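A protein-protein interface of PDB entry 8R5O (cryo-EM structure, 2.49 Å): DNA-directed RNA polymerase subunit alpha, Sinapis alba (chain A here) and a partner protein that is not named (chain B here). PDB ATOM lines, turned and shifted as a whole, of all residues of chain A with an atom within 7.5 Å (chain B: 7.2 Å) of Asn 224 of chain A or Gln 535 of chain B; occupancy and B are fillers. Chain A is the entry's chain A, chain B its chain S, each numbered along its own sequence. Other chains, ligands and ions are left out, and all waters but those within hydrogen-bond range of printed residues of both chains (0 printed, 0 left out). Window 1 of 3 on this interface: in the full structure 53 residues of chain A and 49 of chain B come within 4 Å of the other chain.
The indole nitrogen of Trp 531 of chain B sits at hydrogen-bond distance from the side-chain amide oxygen of Asn 224 of chain A, 3.3 Å away.
NE2 of Gln 535 of chain B sits at hydrogen-bond distance from OD1 of Asn 224 of chain A (3.1 Å).
A ring nitrogen (NE2) of His 231 of chain A lies within hydrogen-bond range of the side-chain amide oxygen (OE1) of Gln 535 of chain B, 2.6 Å away.
O of Arg 220 of chain A lies within hydrogen-bond range of ND2 of Asn 224 of chain A, at 2.9 Å.
O of Leu 532 of chain B lies close to OG1 of Thr 536 of chain B, at 3.4 Å.
The side-chain hydroxyl (OG1) of Thr 536 of chain B sits at hydrogen-bond distance from the backbone carbonyl oxygen (O) of Leu 533 of chain B (2.8 Å).
Trp 531 of chain B touches Arg 220 of chain A.
CG2 of Ile 223 of chain A touches CZ2 of Trp 531 of chain B, 3.8 Å away.
CD1 of Trp 531 of chain B touches CD1 of Ile 227 of chain A, 3.6 Å away.
CD2 of Leu 532 of chain B touches CG1 of Ile 227 of chain A (3.7 Å).
NE2 of Gln 535 of chain B touches CG2 of Ile 227 of chain A (3.6 Å).
His 231 of chain A touches Leu 532 of chain B (NE2 to CD2, 3.5 Å).
Thr 536 of chain B touches His 231 of chain A.
Thr 536 of chain B touches Thr 247 of chain A (O to CA, 3.6 Å).
Thr 247 of chain A touches Arg 537 of chain B (CG2 to O, 3.7 Å).
Of chain B, only Trp 531 and Gln 535 come within 4 Å of Asn 224 of chain A.
Of chain A, only Asn 224, Ile 227 and His 231 come within 4 Å of Gln 535 of chain B.
No residue of chain A comes within 4 Å of Ala 534 of chain B.
Of the printed residues of chain A, Thr 536 of chain B touches His 231 and Thr 247.
Of the printed residues of chain A, Arg 537 of chain B touches Thr 247 (3.7 Å).
Of the printed residues of chain B, Ile 227 of chain A touches Trp 531, Leu 532 and Gln 535.
Of the printed residues of chain B, Thr 247 of chain A touches Thr 536 and Arg 537.
Of the printed residues of chain B, Ile 223 of chain A touches Trp 531 (3.8 Å).
Tyr 539 of chain B touches none of the printed residues of chain A.
Printed residues of chain A that touch a printed residue of chain B: Arg 220, Ile 223, Asn 224, Ile 227, His 231 and Thr 247.
Hydrophobic or aromatic side chains of chain A that line the printed part of chain B: Ile 223, Ile 227 and His 231.
Of the 16 printed residues of chain B, 5 touch a printed residue of chain A.
Printed residues of chain B that touch a printed residue of chain A: Trp 531, Leu 532, Gln 535, Thr 536 and Arg 537.
Among the printed residues, no Asp or Glu carboxylate lies within 4 Å of a Lys or Arg side-chain nitrogen of the other chain.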
ATOM      1  N   GLU A 217     -19.615  18.987 -20.717  1.00  0.00           N
ATOM      2  CA  GLU A 217     -20.218  17.799 -20.125  1.00  0.00           C
ATOM      3  C   GLU A 217     -21.232  17.163 -21.068  1.00  0.00           C
ATOM      4  O   GLU A 217     -21.308  15.933 -21.166  1.00  0.00           O
ATOM      5  CB  GLU A 217     -20.875  18.144 -18.789  1.00  0.00           C
ATOM      6  CG  GLU A 217     -21.433  16.934 -18.060  1.00  0.00           C
ATOM      7  CD  GLU A 217     -22.134  17.299 -16.769  1.00  0.00           C
ATOM      8  OE1 GLU A 217     -22.068  18.478 -16.366  1.00  0.00           O
ATOM      9  OE2 GLU A 217     -22.754  16.402 -16.156  1.00  0.00           O
ATOM     10  N   ALA A 218     -22.023  17.980 -21.763  1.00  0.00           N
ATOM     11  CA  ALA A 218     -22.978  17.442 -22.724  1.00  0.00           C
ATOM     12  C   ALA A 218     -22.267  16.718 -23.860  1.00  0.00           C
ATOM     13  O   ALA A 218     -22.718  15.659 -24.309  1.00  0.00           O
ATOM     14  CB  ALA A 218     -23.869  18.558 -23.266  1.00  0.00           C
ATOM     15  N   SER A 219     -21.152  17.277 -24.338  1.00  0.00           N
ATOM     16  CA  SER A 219     -20.382  16.612 -25.386  1.00  0.00           C
ATOM     17  C   SER A 219     -19.841  15.270 -24.907  1.00  0.00           C
ATOM     18  O   SER A 219     -19.903  14.273 -25.634  1.00  0.00           O
ATOM     19  CB  SER A 219     -19.239  17.512 -25.851  1.00  0.00           C
ATOM     20  OG  SER A 219     -19.729  18.734 -26.374  1.00  0.00           O
ATOM     21  N   ARG A 220     -19.302  15.224 -23.686  1.00  0.00           N
ATOM     22  CA  ARG A 220     -18.807  13.963 -23.143  1.00  0.00           C
ATOM     23  C   ARG A 220     -19.937  12.968 -22.923  1.00  0.00           C
ATOM     24  O   ARG A 220     -19.772  11.770 -23.178  1.00  0.00           O
ATOM     25  CB  ARG A 220     -18.056  14.204 -21.839  1.00  0.00           C
ATOM     26  CG  ARG A 220     -16.750  14.929 -22.020  1.00  0.00           C
ATOM     27  CD  ARG A 220     -15.986  15.020 -20.719  1.00  0.00           C
ATOM     28  NE  ARG A 220     -14.666  15.590 -20.941  1.00  0.00           N
ATOM     29  CZ  ARG A 220     -13.602  14.887 -21.296  1.00  0.00           C
ATOM     30  NH1 ARG A 220     -13.656  13.573 -21.436  1.00  0.00           N
ATOM     31  NH2 ARG A 220     -12.455  15.519 -21.521  1.00  0.00           N
ATOM     32  N   ASN A 221     -21.081  13.438 -22.423  1.00  0.00           N
ATOM     33  CA  ASN A 221     -22.212  12.540 -22.215  1.00  0.00           C
ATOM     34  C   ASN A 221     -22.714  11.978 -23.538  1.00  0.00           C
ATOM     35  O   ASN A 221     -23.077  10.799 -23.620  1.00  0.00           O
ATOM     36  CB  ASN A 221     -23.334  13.263 -21.472  1.00  0.00           C
ATOM     37  CG  ASN A 221     -22.971  13.580 -20.034  1.00  0.00           C
ATOM     38  OD1 ASN A 221     -22.003  13.046 -19.494  1.00  0.00           O
ATOM     39  ND2 ASN A 221     -23.751  14.448 -19.404  1.00  0.00           N
ATOM     40  N   LEU A 222     -22.741  12.806 -24.585  1.00  0.00           N
ATOM     41  CA  LEU A 222     -23.167  12.332 -25.897  1.00  0.00           C
ATOM     42  C   LEU A 222     -22.232  11.256 -26.431  1.00  0.00           C
ATOM     43  O   LEU A 222     -22.684  10.260 -27.004  1.00  0.00           O
ATOM     44  CB  LEU A 222     -23.252  13.503 -26.874  1.00  0.00           C
ATOM     45  CG  LEU A 222     -24.469  14.414 -26.733  1.00  0.00           C
ATOM     46  CD1 LEU A 222     -24.291  15.682 -27.546  1.00  0.00           C
ATOM     47  CD2 LEU A 222     -25.726  13.680 -27.160  1.00  0.00           C
ATOM     48  N   ILE A 223     -20.923  11.438 -26.250  1.00  0.00           N
ATOM     49  CA  ILE A 223     -19.961  10.453 -26.738  1.00  0.00           C
ATOM     50  C   ILE A 223     -20.169   9.114 -26.045  1.00  0.00           C
ATOM     51  O   ILE A 223     -20.173   8.059 -26.692  1.00  0.00           O
ATOM     52  CB  ILE A 223     -18.525  10.979 -26.562  1.00  0.00           C
ATOM     53  CG1 ILE A 223     -18.294  12.185 -27.473  1.00  0.00           C
ATOM     54  CG2 ILE A 223     -17.513   9.885 -26.852  1.00  0.00           C
ATOM     55  CD1 ILE A 223     -16.960  12.852 -27.285  1.00  0.00           C
ATOM     56  N   ASN A 224     -20.367   9.131 -24.725  1.00  0.00           N
ATOM     57  CA  ASN A 224     -20.607   7.899 -23.982  1.00  0.00           C
ATOM     58  C   ASN A 224     -21.937   7.242 -24.337  1.00  0.00           C
ATOM     59  O   ASN A 224     -22.140   6.073 -23.999  1.00  0.00           O
ATOM     60  CB  ASN A 224     -20.555   8.166 -22.477  1.00  0.00           C
ATOM     61  CG  ASN A 224     -19.142   8.351 -21.967  1.00  0.00           C
ATOM     62  OD1 ASN A 224     -18.379   7.392 -21.870  1.00  0.00           O
ATOM     63  ND2 ASN A 224     -18.791   9.583 -21.626  1.00  0.00           N
ATOM     64  N   LEU A 225     -22.845   7.962 -24.991  1.00  0.00           N
ATOM     65  CA  LEU A 225     -24.092   7.371 -25.457  1.00  0.00           C
ATOM     66  C   LEU A 225     -23.958   6.712 -26.822  1.00  0.00           C
ATOM     67  O   LEU A 225     -24.727   5.794 -27.137  1.00  0.00           O
ATOM     68  CB  LEU A 225     -25.195   8.430 -25.518  1.00  0.00           C
ATOM     69  CG  LEU A 225     -25.798   8.891 -24.192  1.00  0.00           C
ATOM     70  CD1 LEU A 225     -26.806  10.002 -24.426  1.00  0.00           C
ATOM     71  CD2 LEU A 225     -26.445   7.723 -23.468  1.00  0.00           C
ATOM     72  N   PHE A 226     -23.006   7.158 -27.639  1.00  0.00           N
ATOM     73  CA  PHE A 226     -22.821   6.636 -28.987  1.00  0.00           C
ATOM     74  C   PHE A 226     -21.716   5.596 -29.082  1.00  0.00           C
ATOM     75  O   PHE A 226     -21.759   4.740 -29.969  1.00  0.00           O
ATOM     76  CB  PHE A 226     -22.515   7.782 -29.957  1.00  0.00           C
ATOM     77  CG  PHE A 226     -23.565   8.856 -29.976  1.00  0.00           C
ATOM     78  CD1 PHE A 226     -24.907   8.533 -29.885  1.00  0.00           C
ATOM     79  CD2 PHE A 226     -23.207  10.190 -30.081  1.00  0.00           C
ATOM     80  CE1 PHE A 226     -25.871   9.517 -29.901  1.00  0.00           C
ATOM     81  CE2 PHE A 226     -24.169  11.180 -30.096  1.00  0.00           C
ATOM     82  CZ  PHE A 226     -25.503  10.842 -30.004  1.00  0.00           C
ATOM     83  N   ILE A 227     -20.734   5.652 -28.189  1.00  0.00           N
ATOM     84  CA  ILE A 227     -19.590   4.743 -28.197  1.00  0.00           C
ATOM     85  C   ILE A 227     -19.937   3.288 -27.869  1.00  0.00           C
ATOM     86  O   ILE A 227     -19.156   2.403 -28.249  1.00  0.00           O
ATOM     87  CB  ILE A 227     -18.480   5.266 -27.268  1.00  0.00           C
ATOM     88  CG1 ILE A 227     -17.111   4.917 -27.853  1.00  0.00           C
ATOM     89  CG2 ILE A 227     -18.617   4.710 -25.862  1.00  0.00           C
ATOM     90  CD1 ILE A 227     -15.954   5.527 -27.111  1.00  0.00           C
ATOM     91  N   PRO A 228     -21.034   2.959 -27.163  1.00  0.00           N
ATOM     92  CA  PRO A 228     -21.326   1.528 -26.954  1.00  0.00           C
ATOM     93  C   PRO A 228     -21.460   0.732 -28.238  1.00  0.00           C
ATOM     94  O   PRO A 228     -21.132  -0.460 -28.246  1.00  0.00           O
ATOM     95  CB  PRO A 228     -22.642   1.553 -26.166  1.00  0.00           C
ATOM     96  CG  PRO A 228     -22.581   2.803 -25.420  1.00  0.00           C
ATOM     97  CD  PRO A 228     -21.939   3.788 -26.342  1.00  0.00           C
ATOM     98  N   PHE A 229     -21.928   1.348 -29.325  1.00  0.00           N
ATOM     99  CA  PHE A 229     -21.989   0.653 -30.605  1.00  0.00           C
ATOM    100  C   PHE A 229     -20.612   0.299 -31.153  1.00  0.00           C
ATOM    101  O   PHE A 229     -20.525  -0.535 -32.060  1.00  0.00           O
ATOM    102  CB  PHE A 229     -22.740   1.493 -31.636  1.00  0.00           C
ATOM    103  CG  PHE A 229     -24.199   1.666 -31.334  1.00  0.00           C
ATOM    104  CD1 PHE A 229     -25.058   0.582 -31.365  1.00  0.00           C
ATOM    105  CD2 PHE A 229     -24.714   2.917 -31.042  1.00  0.00           C
ATOM    106  CE1 PHE A 229     -26.401   0.739 -31.095  1.00  0.00           C
ATOM    107  CE2 PHE A 229     -26.057   3.080 -30.773  1.00  0.00           C
ATOM    108  CZ  PHE A 229     -26.901   1.989 -30.800  1.00  0.00           C
ATOM    109  N   HIS A 231     -18.134  -0.916 -29.148  1.00  0.00           N
ATOM    110  CA  HIS A 231     -17.684  -2.121 -28.474  1.00  0.00           C
ATOM    111  C   HIS A 231     -18.014  -3.345 -29.321  1.00  0.00           C
ATOM    112  O   HIS A 231     -18.825  -3.287 -30.249  1.00  0.00           O
ATOM    113  CB  HIS A 231     -18.338  -2.257 -27.099  1.00  0.00           C
ATOM    114  CG  HIS A 231     -17.732  -1.383 -26.048  1.00  0.00           C
ATOM    115  ND1 HIS A 231     -16.477  -1.612 -25.524  1.00  0.00           N
ATOM    116  CD2 HIS A 231     -18.210  -0.287 -25.415  1.00  0.00           C
ATOM    117  CE1 HIS A 231     -16.209  -0.691 -24.618  1.00  0.00           C
ATOM    118  NE2 HIS A 231     -17.242   0.127 -24.533  1.00  0.00           N
ATOM    119  N   THR A 247     -12.997  -7.725 -17.940  1.00  0.00           N
ATOM    120  CA  THR A 247     -11.794  -6.910 -17.818  1.00  0.00           C
ATOM    121  C   THR A 247     -10.751  -7.336 -18.847  1.00  0.00           C
ATOM    122  O   THR A 247     -10.184  -6.505 -19.550  1.00  0.00           O
ATOM    123  CB  THR A 247     -11.188  -7.001 -16.402  1.00  0.00           C
ATOM    124  OG1 THR A 247     -12.193  -6.691 -15.432  1.00  0.00           O
ATOM    125  CG2 THR A 247     -10.034  -6.024 -16.246  1.00  0.00           C
ATOM    126  N   PRO B 479     -10.869   9.600 -21.181  1.00  0.00           N
ATOM    127  CA  PRO B 479     -10.896   8.922 -19.879  1.00  0.00           C
ATOM    128  C   PRO B 479      -9.758   7.919 -19.779  1.00  0.00           C
ATOM    129  O   PRO B 479      -9.598   7.046 -20.634  1.00  0.00           O
ATOM    130  CB  PRO B 479     -12.265   8.233 -19.863  1.00  0.00           C
ATOM    131  CG  PRO B 479     -13.075   8.949 -20.891  1.00  0.00           C
ATOM    132  CD  PRO B 479     -12.108   9.374 -21.945  1.00  0.00           C
ATOM    133  N   THR B 481      -7.586   5.359 -16.921  1.00  0.00           N
ATOM    134  CA  THR B 481      -7.616   4.679 -15.634  1.00  0.00           C
ATOM    135  C   THR B 481      -6.205   4.197 -15.319  1.00  0.00           C
ATOM    136  O   THR B 481      -5.333   4.242 -16.195  1.00  0.00           O
ATOM    137  CB  THR B 481      -8.605   3.512 -15.666  1.00  0.00           C
ATOM    138  OG1 THR B 481      -8.024   2.410 -16.372  1.00  0.00           O
ATOM    139  CG2 THR B 481      -9.891   3.916 -16.366  1.00  0.00           C
ATOM    140  N   THR B 484      -5.012   1.721 -17.900  1.00  0.00           N
ATOM    141  CA  THR B 484      -4.814   2.154 -19.280  1.00  0.00           C
ATOM    142  C   THR B 484      -3.887   3.358 -19.395  1.00  0.00           C
ATOM    143  O   THR B 484      -3.851   3.997 -20.451  1.00  0.00           O
ATOM    144  CB  THR B 484      -6.159   2.486 -19.942  1.00  0.00           C
ATOM    145  OG1 THR B 484      -6.743   3.623 -19.296  1.00  0.00           O
ATOM    146  CG2 THR B 484      -7.118   1.316 -19.849  1.00  0.00           C
ATOM    147  N   GLN B 530      -8.631   4.405 -27.245  1.00  0.00           N
ATOM    148  CA  GLN B 530      -8.294   4.688 -25.853  1.00  0.00           C
ATOM    149  C   GLN B 530      -9.550   4.799 -24.998  1.00  0.00           C
ATOM    150  O   GLN B 530      -9.597   4.280 -23.877  1.00  0.00           O
ATOM    151  CB  GLN B 530      -7.478   5.974 -25.764  1.00  0.00           C
ATOM    152  CG  GLN B 530      -6.899   6.234 -24.396  1.00  0.00           C
ATOM    153  CD  GLN B 530      -5.881   5.188 -24.001  1.00  0.00           C
ATOM    154  OE1 GLN B 530      -5.000   4.839 -24.783  1.00  0.00           O
ATOM    155  NE2 GLN B 530      -6.004   4.674 -22.788  1.00  0.00           N
ATOM    156  N   TRP B 531     -10.578   5.472 -25.516  1.00  0.00           N
ATOM    157  CA  TRP B 531     -11.826   5.642 -24.782  1.00  0.00           C
ATOM    158  C   TRP B 531     -12.485   4.298 -24.495  1.00  0.00           C
ATOM    159  O   TRP B 531     -12.989   4.069 -23.390  1.00  0.00           O
ATOM    160  CB  TRP B 531     -12.766   6.543 -25.583  1.00  0.00           C
ATOM    161  CG  TRP B 531     -13.778   7.286 -24.778  1.00  0.00           C
ATOM    162  CD1 TRP B 531     -14.719   6.756 -23.955  1.00  0.00           C
ATOM    163  CD2 TRP B 531     -13.974   8.703 -24.755  1.00  0.00           C
ATOM    164  NE1 TRP B 531     -15.482   7.755 -23.403  1.00  0.00           N
ATOM    165  CE2 TRP B 531     -15.045   8.961 -23.881  1.00  0.00           C
ATOM    166  CE3 TRP B 531     -13.343   9.780 -25.383  1.00  0.00           C
ATOM    167  CZ2 TRP B 531     -15.496  10.251 -23.615  1.00  0.00           C
ATOM    168  CZ3 TRP B 531     -13.791  11.056 -25.120  1.00  0.00           C
ATOM    169  CH2 TRP B 531     -14.858  11.282 -24.246  1.00  0.00           C
ATOM    170  N   LEU B 532     -12.493   3.399 -25.482  1.00  0.00           N
ATOM    171  CA  LEU B 532     -13.097   2.084 -25.290  1.00  0.00           C
ATOM    172  C   LEU B 532     -12.338   1.263 -24.255  1.00  0.00           C
ATOM    173  O   LEU B 532     -12.949   0.564 -23.439  1.00  0.00           O
ATOM    174  CB  LEU B 532     -13.154   1.334 -26.622  1.00  0.00           C
ATOM    175  CG  LEU B 532     -14.126   1.850 -27.682  1.00  0.00           C
ATOM    176  CD1 LEU B 532     -13.877   1.157 -29.008  1.00  0.00           C
ATOM    177  CD2 LEU B 532     -15.563   1.643 -27.232  1.00  0.00           C
ATOM    178  N   LEU B 533     -11.006   1.330 -24.273  1.00  0.00           N
ATOM    179  CA  LEU B 533     -10.215   0.504 -23.366  1.00  0.00           C
ATOM    180  C   LEU B 533     -10.452   0.878 -21.908  1.00  0.00           C
ATOM    181  O   LEU B 533     -10.402   0.008 -21.033  1.00  0.00           O
ATOM    182  CB  LEU B 533      -8.732   0.607 -23.708  1.00  0.00           C
ATOM    183  CG  LEU B 533      -7.845  -0.430 -23.015  1.00  0.00           C
ATOM    184  CD1 LEU B 533      -8.202  -1.834 -23.478  1.00  0.00           C
ATOM    185  CD2 LEU B 533      -6.373  -0.145 -23.242  1.00  0.00           C
ATOM    186  N   ALA B 534     -10.706   2.157 -21.627  1.00  0.00           N
ATOM    187  CA  ALA B 534     -11.017   2.566 -20.261  1.00  0.00           C
ATOM    188  C   ALA B 534     -12.308   1.922 -19.774  1.00  0.00           C
ATOM    189  O   ALA B 534     -12.401   1.494 -18.619  1.00  0.00           O
ATOM    190  CB  ALA B 534     -11.116   4.087 -20.174  1.00  0.00           C
ATOM    191  N   GLN B 535     -13.319   1.853 -20.640  1.00  0.00           N
ATOM    192  CA  GLN B 535     -14.578   1.222 -20.258  1.00  0.00           C
ATOM    193  C   GLN B 535     -14.406  -0.276 -20.039  1.00  0.00           C
ATOM    194  O   GLN B 535     -14.950  -0.833 -19.079  1.00  0.00           O
ATOM    195  CB  GLN B 535     -15.645   1.500 -21.320  1.00  0.00           C
ATOM    196  CG  GLN B 535     -15.997   2.973 -21.464  1.00  0.00           C
ATOM    197  CD  GLN B 535     -17.151   3.222 -22.417  1.00  0.00           C
ATOM    198  OE1 GLN B 535     -17.563   2.334 -23.162  1.00  0.00           O
ATOM    199  NE2 GLN B 535     -17.682   4.436 -22.393  1.00  0.00           N
ATOM    200  N   THR B 536     -13.649  -0.944 -20.914  1.00  0.00           N
ATOM    201  CA  THR B 536     -13.479  -2.390 -20.791  1.00  0.00           C
ATOM    202  C   THR B 536     -12.711  -2.763 -19.527  1.00  0.00           C
ATOM    203  O   THR B 536     -13.100  -3.695 -18.815  1.00  0.00           O
ATOM    204  CB  THR B 536     -12.770  -2.950 -22.025  1.00  0.00           C
ATOM    205  OG1 THR B 536     -11.505  -2.301 -22.190  1.00  0.00           O
ATOM    206  CG2 THR B 536     -13.610  -2.734 -23.273  1.00  0.00           C
ATOM    207  N   ARG B 537     -11.624  -2.051 -19.229  1.00  0.00           N
ATOM    208  CA  ARG B 537     -10.768  -2.451 -18.114  1.00  0.00           C
ATOM    209  C   ARG B 537     -11.253  -1.894 -16.781  1.00  0.00           C
ATOM    210  O   ARG B 537     -11.159  -2.577 -15.755  1.00  0.00           O
ATOM    211  CB  ARG B 537      -9.328  -2.019 -18.377  1.00  0.00           C
ATOM    212  CG  ARG B 537      -8.625  -2.876 -19.405  1.00  0.00           C
ATOM    213  CD  ARG B 537      -7.163  -2.515 -19.528  1.00  0.00           C
ATOM    214  NE  ARG B 537      -6.480  -3.390 -20.468  1.00  0.00           N
ATOM    215  CZ  ARG B 537      -5.244  -3.201 -20.909  1.00  0.00           C
ATOM    216  NH1 ARG B 537      -4.508  -2.185 -20.492  1.00  0.00           N
ATOM    217  NH2 ARG B 537      -4.737  -4.050 -21.797  1.00  0.00           N
ATOM    218  N   GLY B 538     -11.767  -0.667 -16.769  1.00  0.00           N
ATOM    219  CA  GLY B 538     -12.218  -0.091 -15.519  1.00  0.00           C
ATOM    220  C   GLY B 538     -11.070   0.371 -14.631  1.00  0.00           C
ATOM    221  O   GLY B 538      -9.959   0.647 -15.083  1.00  0.00           O
ATOM    222  N   TYR B 539     -11.364   0.439 -13.332  1.00  0.00           N
ATOM    223  CA  TYR B 539     -10.470   0.975 -12.317  1.00  0.00           C
ATOM    224  C   TYR B 539     -10.128  -0.083 -11.277  1.00  0.00           C
ATOM    225  O   TYR B 539     -10.947  -0.957 -10.983  1.00  0.00           O
ATOM    226  CB  TYR B 539     -11.101   2.174 -11.596  1.00  0.00           C
ATOM    227  CG  TYR B 539     -11.308   3.405 -12.441  1.00  0.00           C
ATOM    228  CD1 TYR B 539     -12.382   3.501 -13.314  1.00  0.00           C
ATOM    229  CD2 TYR B 539     -10.444   4.488 -12.345  1.00  0.00           C
ATOM    230  CE1 TYR B 539     -12.580   4.631 -14.080  1.00  0.00           C
ATOM    231  CE2 TYR B 539     -10.637   5.622 -13.107  1.00  0.00           C
ATOM    232  CZ  TYR B 539     -11.706   5.689 -13.972  1.00  0.00           C
ATOM    233  OH  TYR B 539     -11.897   6.816 -14.732  1.00  0.00           O
ATOM    234  N   ILE B 567     -13.522  -2.066 -10.900  1.00  0.00           N
ATOM    235  CA  ILE B 567     -14.789  -1.400 -10.654  1.00  0.00           C
ATOM    236  C   ILE B 567     -15.056  -0.455 -11.816  1.00  0.00           C
ATOM    237  O   ILE B 567     -14.144  -0.054 -12.542  1.00  0.00           O
ATOM    238  CB  ILE B 567     -14.798  -0.626  -9.317  1.00  0.00           C
ATOM    239  CG1 ILE B 567     -13.768   0.502  -9.355  1.00  0.00           C
ATOM    240  CG2 ILE B 567     -14.527  -1.561  -8.150  1.00  0.00           C
ATOM    241  CD1 ILE B 567     -13.755   1.363  -8.119  1.00  0.00           C
ATOM    242  N   THR B 568     -16.326  -0.105 -11.996  1.00  0.00           N
ATOM    243  CA  THR B 568     -16.678   0.817 -13.060  1.00  0.00           C
ATOM    244  C   THR B 568     -16.352   2.250 -12.648  1.00  0.00           C
ATOM    245  O   THR B 568     -16.094   2.552 -11.482  1.00  0.00           O
ATOM    246  CB  THR B 568     -18.159   0.697 -13.424  1.00  0.00           C
ATOM    247  OG1 THR B 568     -18.961   1.221 -12.360  1.00  0.00           O
ATOM    248  CG2 THR B 568     -18.537  -0.756 -13.667  1.00  0.00           C
ATOM    249  N   GLU B 569     -16.351   3.143 -13.639  1.00  0.00           N
ATOM    250  CA  GLU B 569     -16.130   4.557 -13.363  1.00  0.00           C
ATOM    251  C   GLU B 569     -17.251   5.145 -12.518  1.00  0.00           C
ATOM    252  O   GLU B 569     -17.021   6.099 -11.767  1.00  0.00           O
ATOM    253  CB  GLU B 569     -15.984   5.332 -14.672  1.00  0.00           C
ATOM    254  CG  GLU B 569     -17.118   5.124 -15.663  1.00  0.00           C
ATOM    255  CD  GLU B 569     -16.968   3.855 -16.492  1.00  0.00           C
ATOM    256  OE1 GLU B 569     -16.083   3.029 -16.180  1.00  0.00           O
ATOM    257  OE2 GLU B 569     -17.739   3.684 -17.461  1.00  0.00           O
